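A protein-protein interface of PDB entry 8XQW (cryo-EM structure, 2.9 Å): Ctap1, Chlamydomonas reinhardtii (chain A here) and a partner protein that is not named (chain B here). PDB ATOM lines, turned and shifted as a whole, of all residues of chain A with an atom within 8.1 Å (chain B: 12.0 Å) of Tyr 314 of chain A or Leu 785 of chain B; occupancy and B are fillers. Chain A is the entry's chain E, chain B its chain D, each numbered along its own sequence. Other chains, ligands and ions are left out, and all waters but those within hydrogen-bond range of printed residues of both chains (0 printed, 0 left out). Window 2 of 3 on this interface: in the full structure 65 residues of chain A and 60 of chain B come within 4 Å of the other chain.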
ATOM      1  N   GLN A 164      -7.813 -28.772   3.540  1.00  0.00           N
ATOM      2  CA  GLN A 164      -8.030 -27.629   4.400  1.00  0.00           C
ATOM      3  C   GLN A 164      -7.197 -27.769   5.666  1.00  0.00           C
ATOM      4  O   GLN A 164      -6.859 -28.871   6.094  1.00  0.00           O
ATOM      5  CB  GLN A 164      -9.515 -27.499   4.706  1.00  0.00           C
ATOM      6  CG  GLN A 164     -10.336 -27.774   3.461  1.00  0.00           C
ATOM      7  CD  GLN A 164     -11.666 -27.094   3.455  1.00  0.00           C
ATOM      8  OE1 GLN A 164     -12.163 -26.667   4.482  1.00  0.00           O
ATOM      9  NE2 GLN A 164     -12.258 -26.987   2.283  1.00  0.00           N
ATOM     10  N   GLU A 165      -6.856 -26.625   6.253  1.00  0.00           N
ATOM     11  CA  GLU A 165      -5.922 -26.578   7.369  1.00  0.00           C
ATOM     12  C   GLU A 165      -6.344 -27.525   8.482  1.00  0.00           C
ATOM     13  O   GLU A 165      -7.532 -27.780   8.680  1.00  0.00           O
ATOM     14  CB  GLU A 165      -5.823 -25.143   7.878  1.00  0.00           C
ATOM     15  CG  GLU A 165      -5.184 -24.967   9.231  1.00  0.00           C
ATOM     16  CD  GLU A 165      -3.692 -25.209   9.211  1.00  0.00           C
ATOM     17  OE1 GLU A 165      -3.273 -26.365   8.998  1.00  0.00           O
ATOM     18  OE2 GLU A 165      -2.931 -24.238   9.396  1.00  0.00           O
ATOM     19  N   LEU A 204      -6.574 -14.936  10.228  1.00  0.00           N
ATOM     20  CA  LEU A 204      -7.709 -15.560  10.884  1.00  0.00           C
ATOM     21  C   LEU A 204      -8.133 -16.788  10.101  1.00  0.00           C
ATOM     22  O   LEU A 204      -8.364 -16.709   8.892  1.00  0.00           O
ATOM     23  CB  LEU A 204      -8.881 -14.595  10.988  1.00  0.00           C
ATOM     24  CG  LEU A 204      -8.558 -13.203  11.496  1.00  0.00           C
ATOM     25  CD1 LEU A 204      -9.828 -12.452  11.704  1.00  0.00           C
ATOM     26  CD2 LEU A 204      -7.827 -13.314  12.786  1.00  0.00           C
ATOM     27  N   GLN A 205      -8.235 -17.913  10.791  1.00  0.00           N
ATOM     28  CA  GLN A 205      -8.822 -19.122  10.227  1.00  0.00           C
ATOM     29  C   GLN A 205     -10.067 -19.444  11.036  1.00  0.00           C
ATOM     30  O   GLN A 205      -9.977 -19.679  12.241  1.00  0.00           O
ATOM     31  CB  GLN A 205      -7.832 -20.274  10.261  1.00  0.00           C
ATOM     32  CG  GLN A 205      -6.733 -20.170   9.242  1.00  0.00           C
ATOM     33  CD  GLN A 205      -5.461 -20.836   9.698  1.00  0.00           C
ATOM     34  OE1 GLN A 205      -4.999 -20.615  10.811  1.00  0.00           O
ATOM     35  NE2 GLN A 205      -4.886 -21.659   8.840  1.00  0.00           N
ATOM     36  N   VAL A 206     -11.211 -19.453  10.396  1.00  0.00           N
ATOM     37  CA  VAL A 206     -12.481 -19.643  11.078  1.00  0.00           C
ATOM     38  C   VAL A 206     -12.955 -21.071  10.873  1.00  0.00           C
ATOM     39  O   VAL A 206     -13.320 -21.462   9.763  1.00  0.00           O
ATOM     40  CB  VAL A 206     -13.514 -18.632  10.562  1.00  0.00           C
ATOM     41  CG1 VAL A 206     -14.834 -18.857  11.224  1.00  0.00           C
ATOM     42  CG2 VAL A 206     -13.032 -17.229  10.814  1.00  0.00           C
ATOM     43  N   PHE A 207     -12.952 -21.858  11.943  1.00  0.00           N
ATOM     44  CA  PHE A 207     -13.265 -23.273  11.903  1.00  0.00           C
ATOM     45  C   PHE A 207     -14.687 -23.515  12.364  1.00  0.00           C
ATOM     46  O   PHE A 207     -15.142 -22.916  13.345  1.00  0.00           O
ATOM     47  CB  PHE A 207     -12.351 -24.065  12.815  1.00  0.00           C
ATOM     48  CG  PHE A 207     -11.005 -24.323  12.255  1.00  0.00           C
ATOM     49  CD1 PHE A 207     -10.763 -25.439  11.505  1.00  0.00           C
ATOM     50  CD2 PHE A 207      -9.973 -23.469  12.517  1.00  0.00           C
ATOM     51  CE1 PHE A 207      -9.529 -25.675  11.007  1.00  0.00           C
ATOM     52  CE2 PHE A 207      -8.741 -23.708  12.022  1.00  0.00           C
ATOM     53  CZ  PHE A 207      -8.516 -24.806  11.265  1.00  0.00           C
ATOM     54  N   SER A 208     -15.367 -24.418  11.674  1.00  0.00           N
ATOM     55  CA  SER A 208     -16.634 -24.953  12.144  1.00  0.00           C
ATOM     56  C   SER A 208     -16.525 -26.464  12.289  1.00  0.00           C
ATOM     57  O   SER A 208     -15.812 -27.127  11.536  1.00  0.00           O
ATOM     58  CB  SER A 208     -17.771 -24.596  11.198  1.00  0.00           C
ATOM     59  OG  SER A 208     -17.627 -25.277   9.973  1.00  0.00           O
ATOM     60  N   TYR A 222     -18.541 -21.139  16.244  1.00  0.00           N
ATOM     61  CA  TYR A 222     -17.315 -21.016  15.474  1.00  0.00           C
ATOM     62  C   TYR A 222     -16.108 -20.949  16.389  1.00  0.00           C
ATOM     63  O   TYR A 222     -16.216 -20.636  17.573  1.00  0.00           O
ATOM     64  CB  TYR A 222     -17.340 -19.771  14.599  1.00  0.00           C
ATOM     65  CG  TYR A 222     -18.408 -19.816  13.560  1.00  0.00           C
ATOM     66  CD1 TYR A 222     -18.205 -20.461  12.370  1.00  0.00           C
ATOM     67  CD2 TYR A 222     -19.626 -19.225  13.781  1.00  0.00           C
ATOM     68  CE1 TYR A 222     -19.172 -20.513  11.437  1.00  0.00           C
ATOM     69  CE2 TYR A 222     -20.598 -19.272  12.853  1.00  0.00           C
ATOM     70  CZ  TYR A 222     -20.368 -19.914  11.680  1.00  0.00           C
ATOM     71  OH  TYR A 222     -21.352 -19.964  10.730  1.00  0.00           O
ATOM     72  N   LEU A 247     -24.990  -6.209   9.320  1.00  0.00           N
ATOM     73  CA  LEU A 247     -23.585  -6.126   8.962  1.00  0.00           C
ATOM     74  C   LEU A 247     -23.076  -4.699   8.919  1.00  0.00           C
ATOM     75  O   LEU A 247     -21.869  -4.485   9.039  1.00  0.00           O
ATOM     76  CB  LEU A 247     -23.350  -6.784   7.611  1.00  0.00           C
ATOM     77  CG  LEU A 247     -23.724  -8.249   7.469  1.00  0.00           C
ATOM     78  CD1 LEU A 247     -23.674  -8.622   6.025  1.00  0.00           C
ATOM     79  CD2 LEU A 247     -22.777  -9.108   8.241  1.00  0.00           C
ATOM     80  N   TYR A 261     -20.629 -14.154  17.397  1.00  0.00           N
ATOM     81  CA  TYR A 261     -20.074 -14.092  16.060  1.00  0.00           C
ATOM     82  C   TYR A 261     -20.827 -13.143  15.147  1.00  0.00           C
ATOM     83  O   TYR A 261     -20.351 -12.881  14.041  1.00  0.00           O
ATOM     84  CB  TYR A 261     -20.020 -15.475  15.427  1.00  0.00           C
ATOM     85  CG  TYR A 261     -21.274 -16.283  15.521  1.00  0.00           C
ATOM     86  CD1 TYR A 261     -22.356 -16.010  14.718  1.00  0.00           C
ATOM     87  CD2 TYR A 261     -21.356 -17.350  16.380  1.00  0.00           C
ATOM     88  CE1 TYR A 261     -23.487 -16.756  14.791  1.00  0.00           C
ATOM     89  CE2 TYR A 261     -22.483 -18.101  16.460  1.00  0.00           C
ATOM     90  CZ  TYR A 261     -23.545 -17.804  15.660  1.00  0.00           C
ATOM     91  OH  TYR A 261     -24.682 -18.560  15.741  1.00  0.00           O
ATOM     92  N   VAL A 264     -18.574 -10.056  15.289  1.00  0.00           N
ATOM     93  CA  VAL A 264     -17.321 -10.373  14.620  1.00  0.00           C
ATOM     94  C   VAL A 264     -17.513 -10.417  13.113  1.00  0.00           C
ATOM     95  O   VAL A 264     -16.678  -9.917  12.352  1.00  0.00           O
ATOM     96  CB  VAL A 264     -16.763 -11.693  15.167  1.00  0.00           C
ATOM     97  CG1 VAL A 264     -15.718 -12.242  14.244  1.00  0.00           C
ATOM     98  CG2 VAL A 264     -16.196 -11.469  16.541  1.00  0.00           C
ATOM     99  N   PHE A 265     -18.621 -10.992  12.651  1.00  0.00           N
ATOM    100  CA  PHE A 265     -18.854 -11.014  11.214  1.00  0.00           C
ATOM    101  C   PHE A 265     -19.176  -9.630  10.678  1.00  0.00           C
ATOM    102  O   PHE A 265     -18.812  -9.315   9.544  1.00  0.00           O
ATOM    103  CB  PHE A 265     -19.968 -11.989  10.875  1.00  0.00           C
ATOM    104  CG  PHE A 265     -19.566 -13.415  11.004  1.00  0.00           C
ATOM    105  CD1 PHE A 265     -18.236 -13.769  11.014  1.00  0.00           C
ATOM    106  CD2 PHE A 265     -20.510 -14.402  11.117  1.00  0.00           C
ATOM    107  CE1 PHE A 265     -17.861 -15.082  11.135  1.00  0.00           C
ATOM    108  CE2 PHE A 265     -20.134 -15.712  11.233  1.00  0.00           C
ATOM    109  CZ  PHE A 265     -18.811 -16.049  11.245  1.00  0.00           C
ATOM    110  N   LEU A 268     -15.726  -8.105  10.225  1.00  0.00           N
ATOM    111  CA  LEU A 268     -15.045  -8.684   9.074  1.00  0.00           C
ATOM    112  C   LEU A 268     -15.644  -8.190   7.766  1.00  0.00           C
ATOM    113  O   LEU A 268     -14.929  -8.020   6.776  1.00  0.00           O
ATOM    114  CB  LEU A 268     -15.110 -10.201   9.137  1.00  0.00           C
ATOM    115  CG  LEU A 268     -14.021 -10.833   9.980  1.00  0.00           C
ATOM    116  CD1 LEU A 268     -14.254 -12.315  10.078  1.00  0.00           C
ATOM    117  CD2 LEU A 268     -12.684 -10.546   9.363  1.00  0.00           C
ATOM    118  N   TYR A 269     -16.955  -7.972   7.734  1.00  0.00           N
ATOM    119  CA  TYR A 269     -17.585  -7.494   6.511  1.00  0.00           C
ATOM    120  C   TYR A 269     -17.235  -6.043   6.245  1.00  0.00           C
ATOM    121  O   TYR A 269     -17.030  -5.649   5.097  1.00  0.00           O
ATOM    122  CB  TYR A 269     -19.092  -7.667   6.607  1.00  0.00           C
ATOM    123  CG  TYR A 269     -19.886  -6.966   5.539  1.00  0.00           C
ATOM    124  CD1 TYR A 269     -20.185  -7.598   4.350  1.00  0.00           C
ATOM    125  CD2 TYR A 269     -20.373  -5.689   5.735  1.00  0.00           C
ATOM    126  CE1 TYR A 269     -20.915  -6.975   3.383  1.00  0.00           C
ATOM    127  CE2 TYR A 269     -21.106  -5.059   4.771  1.00  0.00           C
ATOM    128  CZ  TYR A 269     -21.377  -5.710   3.598  1.00  0.00           C
ATOM    129  OH  TYR A 269     -22.114  -5.091   2.624  1.00  0.00           O
ATOM    130  N   TYR A 272     -13.441  -4.866   4.735  1.00  0.00           N
ATOM    131  CA  TYR A 272     -13.064  -5.037   3.340  1.00  0.00           C
ATOM    132  C   TYR A 272     -13.748  -4.040   2.424  1.00  0.00           C
ATOM    133  O   TYR A 272     -13.912  -4.316   1.233  1.00  0.00           O
ATOM    134  CB  TYR A 272     -13.373  -6.458   2.889  1.00  0.00           C
ATOM    135  CG  TYR A 272     -12.267  -7.422   3.187  1.00  0.00           C
ATOM    136  CD1 TYR A 272     -11.138  -7.461   2.404  1.00  0.00           C
ATOM    137  CD2 TYR A 272     -12.347  -8.290   4.254  1.00  0.00           C
ATOM    138  CE1 TYR A 272     -10.121  -8.335   2.671  1.00  0.00           C
ATOM    139  CE2 TYR A 272     -11.333  -9.167   4.529  1.00  0.00           C
ATOM    140  CZ  TYR A 272     -10.222  -9.183   3.733  1.00  0.00           C
ATOM    141  OH  TYR A 272      -9.196 -10.052   3.992  1.00  0.00           O
ATOM    142  N   ASP A 311      -5.997 -11.655   6.904  1.00  0.00           N
ATOM    143  CA  ASP A 311      -6.086 -12.762   5.964  1.00  0.00           C
ATOM    144  C   ASP A 311      -7.124 -13.745   6.476  1.00  0.00           C
ATOM    145  O   ASP A 311      -6.844 -14.504   7.403  1.00  0.00           O
ATOM    146  CB  ASP A 311      -4.731 -13.449   5.804  1.00  0.00           C
ATOM    147  CG  ASP A 311      -4.717 -14.465   4.683  1.00  0.00           C
ATOM    148  OD1 ASP A 311      -5.800 -14.902   4.246  1.00  0.00           O
ATOM    149  OD2 ASP A 311      -3.611 -14.830   4.233  1.00  0.00           O
ATOM    150  N   VAL A 312      -8.301 -13.753   5.863  1.00  0.00           N
ATOM    151  CA  VAL A 312      -9.437 -14.511   6.368  1.00  0.00           C
ATOM    152  C   VAL A 312      -9.603 -15.801   5.583  1.00  0.00           C
ATOM    153  O   VAL A 312      -9.551 -15.810   4.352  1.00  0.00           O
ATOM    154  CB  VAL A 312     -10.718 -13.666   6.300  1.00  0.00           C
ATOM    155  CG1 VAL A 312     -11.879 -14.451   6.830  1.00  0.00           C
ATOM    156  CG2 VAL A 312     -10.533 -12.411   7.092  1.00  0.00           C
ATOM    157  N   SER A 313      -9.809 -16.900   6.304  1.00  0.00           N
ATOM    158  CA  SER A 313     -10.036 -18.191   5.676  1.00  0.00           C
ATOM    159  C   SER A 313     -11.127 -18.935   6.422  1.00  0.00           C
ATOM    160  O   SER A 313     -11.336 -18.712   7.610  1.00  0.00           O
ATOM    161  CB  SER A 313      -8.774 -19.038   5.660  1.00  0.00           C
ATOM    162  OG  SER A 313      -7.630 -18.228   5.506  1.00  0.00           O
ATOM    163  N   TYR A 314     -11.804 -19.839   5.723  1.00  0.00           N
ATOM    164  CA  TYR A 314     -12.892 -20.614   6.296  1.00  0.00           C
ATOM    165  C   TYR A 314     -12.600 -22.096   6.158  1.00  0.00           C
ATOM    166  O   TYR A 314     -12.292 -22.568   5.065  1.00  0.00           O
ATOM    167  CB  TYR A 314     -14.206 -20.279   5.617  1.00  0.00           C
ATOM    168  CG  TYR A 314     -14.585 -18.838   5.771  1.00  0.00           C
ATOM    169  CD1 TYR A 314     -15.175 -18.383   6.929  1.00  0.00           C
ATOM    170  CD2 TYR A 314     -14.337 -17.929   4.769  1.00  0.00           C
ATOM    171  CE1 TYR A 314     -15.513 -17.071   7.085  1.00  0.00           C
ATOM    172  CE2 TYR A 314     -14.672 -16.612   4.915  1.00  0.00           C
ATOM    173  CZ  TYR A 314     -15.259 -16.188   6.074  1.00  0.00           C
ATOM    174  OH  TYR A 314     -15.599 -14.870   6.223  1.00  0.00           O
ATOM    175  N   HIS A 315     -12.709 -22.833   7.261  1.00  0.00           N
ATOM    176  CA  HIS A 315     -12.432 -24.258   7.239  1.00  0.00           C
ATOM    177  C   HIS A 315     -13.484 -25.024   8.023  1.00  0.00           C
ATOM    178  O   HIS A 315     -14.155 -24.491   8.911  1.00  0.00           O
ATOM    179  CB  HIS A 315     -11.068 -24.593   7.831  1.00  0.00           C
ATOM    180  CG  HIS A 315      -9.973 -23.688   7.386  1.00  0.00           C
ATOM    181  ND1 HIS A 315      -9.361 -23.807   6.161  1.00  0.00           N
ATOM    182  CD2 HIS A 315      -9.364 -22.657   8.012  1.00  0.00           C
ATOM    183  CE1 HIS A 315      -8.427 -22.883   6.048  1.00  0.00           C
ATOM    184  NE2 HIS A 315      -8.411 -22.170   7.158  1.00  0.00           N
ATOM    185  N   GLY A 316     -13.588 -26.303   7.698  1.00  0.00           N
ATOM    186  CA  GLY A 316     -14.358 -27.254   8.479  1.00  0.00           C
ATOM    187  C   GLY A 316     -13.427 -28.311   9.047  1.00  0.00           C
ATOM    188  O   GLY A 316     -12.646 -28.913   8.313  1.00  0.00           O
ATOM    189  N   THR A 317     -13.500 -28.516  10.355  1.00  0.00           N
ATOM    190  CA  THR A 317     -12.698 -29.538  11.018  1.00  0.00           C
ATOM    191  C   THR A 317     -13.232 -30.890  10.585  1.00  0.00           C
ATOM    192  O   THR A 317     -14.310 -31.304  11.011  1.00  0.00           O
ATOM    193  CB  THR A 317     -12.766 -29.396  12.530  1.00  0.00           C
ATOM    194  OG1 THR A 317     -13.913 -30.101  13.007  1.00  0.00           O
ATOM    195  CG2 THR A 317     -12.891 -27.958  12.910  1.00  0.00           C
ATOM    196  N   ASN B 782     -27.816 -10.994   5.749  1.00  0.00           N
ATOM    197  CA  ASN B 782     -26.519 -11.523   6.140  1.00  0.00           C
ATOM    198  C   ASN B 782     -25.994 -12.533   5.121  1.00  0.00           C
ATOM    199  O   ASN B 782     -25.890 -12.237   3.931  1.00  0.00           O
ATOM    200  CB  ASN B 782     -26.609 -12.166   7.521  1.00  0.00           C
ATOM    201  CG  ASN B 782     -25.255 -12.358   8.164  1.00  0.00           C
ATOM    202  OD1 ASN B 782     -24.347 -12.937   7.569  1.00  0.00           O
ATOM    203  ND2 ASN B 782     -25.108 -11.872   9.387  1.00  0.00           N
ATOM    204  N   GLY B 783     -25.675 -13.724   5.605  1.00  0.00           N
ATOM    205  CA  GLY B 783     -25.104 -14.782   4.796  1.00  0.00           C
ATOM    206  C   GLY B 783     -24.174 -15.625   5.636  1.00  0.00           C
ATOM    207  O   GLY B 783     -23.340 -15.118   6.386  1.00  0.00           O
ATOM    208  N   HIS B 784     -24.332 -16.940   5.509  1.00  0.00           N
ATOM    209  CA  HIS B 784     -23.708 -17.861   6.449  1.00  0.00           C
ATOM    210  C   HIS B 784     -22.461 -18.502   5.863  1.00  0.00           C
ATOM    211  O   HIS B 784     -22.263 -18.535   4.646  1.00  0.00           O
ATOM    212  CB  HIS B 784     -24.675 -18.946   6.917  1.00  0.00           C
ATOM    213  CG  HIS B 784     -25.064 -18.800   8.354  1.00  0.00           C
ATOM    214  ND1 HIS B 784     -24.632 -17.746   9.130  1.00  0.00           N
ATOM    215  CD2 HIS B 784     -25.837 -19.565   9.155  1.00  0.00           C
ATOM    216  CE1 HIS B 784     -25.125 -17.867  10.347  1.00  0.00           C
ATOM    217  NE2 HIS B 784     -25.858 -18.964  10.390  1.00  0.00           N
ATOM    218  N   LEU B 785     -21.623 -19.013   6.767  1.00  0.00           N
ATOM    219  CA  LEU B 785     -20.250 -19.357   6.433  1.00  0.00           C
ATOM    220  C   LEU B 785     -19.865 -20.774   6.831  1.00  0.00           C
ATOM    221  O   LEU B 785     -18.671 -21.051   6.978  1.00  0.00           O
ATOM    222  CB  LEU B 785     -19.303 -18.363   7.097  1.00  0.00           C
ATOM    223  CG  LEU B 785     -19.692 -16.907   6.860  1.00  0.00           C
ATOM    224  CD1 LEU B 785     -18.853 -15.970   7.691  1.00  0.00           C
ATOM    225  CD2 LEU B 785     -19.556 -16.585   5.391  1.00  0.00           C
ATOM    226  N   SER B 786     -20.822 -21.675   7.012  1.00  0.00           N
ATOM    227  CA  SER B 786     -20.490 -23.049   7.347  1.00  0.00           C
ATOM    228  C   SER B 786     -19.820 -23.734   6.167  1.00  0.00           C
ATOM    229  O   SER B 786     -20.224 -23.560   5.017  1.00  0.00           O
ATOM    230  CB  SER B 786     -21.741 -23.826   7.747  1.00  0.00           C
ATOM    231  OG  SER B 786     -22.156 -24.671   6.689  1.00  0.00           O
ATOM    232  N   VAL B 787     -18.793 -24.518   6.457  1.00  0.00           N
ATOM    233  CA  VAL B 787     -18.050 -25.245   5.446  1.00  0.00           C
ATOM    234  C   VAL B 787     -17.772 -26.641   5.976  1.00  0.00           C
ATOM    235  O   VAL B 787     -17.354 -26.815   7.122  1.00  0.00           O
ATOM    236  CB  VAL B 787     -16.739 -24.520   5.085  1.00  0.00           C
ATOM    237  CG1 VAL B 787     -15.809 -25.437   4.351  1.00  0.00           C
ATOM    238  CG2 VAL B 787     -17.027 -23.320   4.240  1.00  0.00           C
ATOM    239  N   VAL B 788     -18.035 -27.638   5.148  1.00  0.00           N
ATOM    240  CA  VAL B 788     -17.703 -29.017   5.460  1.00  0.00           C
ATOM    241  C   VAL B 788     -16.341 -29.307   4.857  1.00  0.00           C
ATOM    242  O   VAL B 788     -15.956 -28.706   3.854  1.00  0.00           O
ATOM    243  CB  VAL B 788     -18.776 -29.979   4.922  1.00  0.00           C
ATOM    244  CG1 VAL B 788     -18.650 -31.329   5.562  1.00  0.00           C
ATOM    245  CG2 VAL B 788     -20.144 -29.415   5.182  1.00  0.00           C
ATOM    246  N   SER B 789     -15.592 -30.212   5.480  1.00  0.00           N
ATOM    247  CA  SER B 789     -14.242 -30.478   4.994  1.00  0.00           C
ATOM    248  C   SER B 789     -14.268 -31.319   3.728  1.00  0.00           C
ATOM    249  O   SER B 789     -13.555 -31.021   2.763  1.00  0.00           O
ATOM    250  CB  SER B 789     -13.420 -31.167   6.074  1.00  0.00           C
ATOM    251  OG  SER B 789     -12.040 -31.103   5.777  1.00  0.00           O
ATOM    252  N   ASN B 790     -15.075 -32.369   3.711  1.00  0.00           N
ATOM    253  CA  ASN B 790     -15.213 -33.218   2.541  1.00  0.00           C
ATOM    254  C   ASN B 790     -16.669 -33.247   2.130  1.00  0.00           C
ATOM    255  O   ASN B 790     -17.524 -33.685   2.902  1.00  0.00           O
ATOM    256  CB  ASN B 790     -14.719 -34.637   2.822  1.00  0.00           C
ATOM    257  CG  ASN B 790     -13.258 -34.810   2.504  1.00  0.00           C
ATOM    258  OD1 ASN B 790     -12.773 -34.309   1.493  1.00  0.00           O
ATOM    259  ND2 ASN B 790     -12.541 -35.512   3.369  1.00  0.00           N
ATOM    260  N   ALA B 791     -16.946 -32.768   0.924  1.00  0.00           N
ATOM    261  CA  ALA B 791     -18.285 -32.872   0.381  1.00  0.00           C
ATOM    262  C   ALA B 791     -18.699 -34.331   0.315  1.00  0.00           C
ATOM    263  O   ALA B 791     -17.971 -35.184  -0.194  1.00  0.00           O
ATOM    264  CB  ALA B 791     -18.353 -32.247  -1.006  1.00  0.00           C
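The backbone carbonyl oxygen (O) of Gly 316 of chain A lies close to the side-chain hydroxyl (OG) of Ser 789 of chain B, at 3.4 Å. O of Val 787 of chain B sits at hydrogen-bond distance from OG of Ser 208 of chain A, at 3.3 Å.
The backbone carbonyl oxygen (O) of His 315 of chain A lies within hydrogen-bond range of the backbone NH (N) of Ser 208 of chain A (3.0 Å). The backbone NH (N) of Thr 317 of chain A lies within hydrogen-bond range of the backbone carbonyl oxygen (O) of Ser 208 of chain A.
Among the printed residues, pairs that only touch across the chains: Gln 164 of chain A with Val 787 of chain B, Leu 247 of chain A with Asn 782 of chain B, Phe 265 of chain A with Leu 785 of chain B, Tyr 314 of chain A with Leu 785 of chain B and Gly 316 of chain A with Val 787 of chain B.
Phe 207 of chain A touches none of the printed residues of chain B. Of the printed residues of chain B, Ser 208 of chain A touches Val 787. Of the printed residues of chain B, Leu 247 of chain A touches Asn 782. No residue of chain B comes within 4 Å of Leu 268 of chain A. No residue of chain B comes within 4 Å of Val 312 of chain A. Ser 313 of chain A touches none of the printed residues of chain B. Of the printed residues of chain B, Tyr 314 of chain A touches Leu 785. His 315 of chain A touches none of the printed residues of chain B. Of chain B, only Val 787 (3.3 Å) and Ser 789 (3.3 Å) come within 4 Å of Gly 316 of chain A. Printed residues of chain A within 4 Å of Asn 782 of chain B: Leu 247 (3.8 Å). Of chain A, only Phe 265 (3.6 Å) and Tyr 314 (3.6 Å) come within 4 Å of Leu 785 of chain B. Ser 786 of chain B touches none of the printed residues of chain A. Printed residues of chain A within 4 Å of Val 787 of chain B: Gln 164, Ser 208 and Gly 316. The nearest printed residue of chain A that does not touch Asn 782 of chain B is Phe 265 of chain A (5.4 Å).
Of the 10 printed residues of chain B, 4 touch a printed residue of chain A. Hydrophobic or aromatic side chains of chain B within 4 Å of the printed part of chain A: Leu 785 and Val 787. Along chain B the printed residues that touch a printed residue of chain A span positions 782 to 789. Of the 22 printed residues of chain A, 6 touch a printed residue of chain B. Printed residues of chain A that touch a printed residue of chain B: Gln 164, Ser 208, Leu 247, Phe 265, Tyr 314 and Gly 316. Hydrophobic or aromatic side chains of chain A within 4 Å of the printed part of chain B: Leu 247, Phe 265 and Tyr 314. Among the printed residues, no Asp or Glu carboxylate lies within 4 Å of a Lys or Arg side-chain nitrogen of the other chain.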
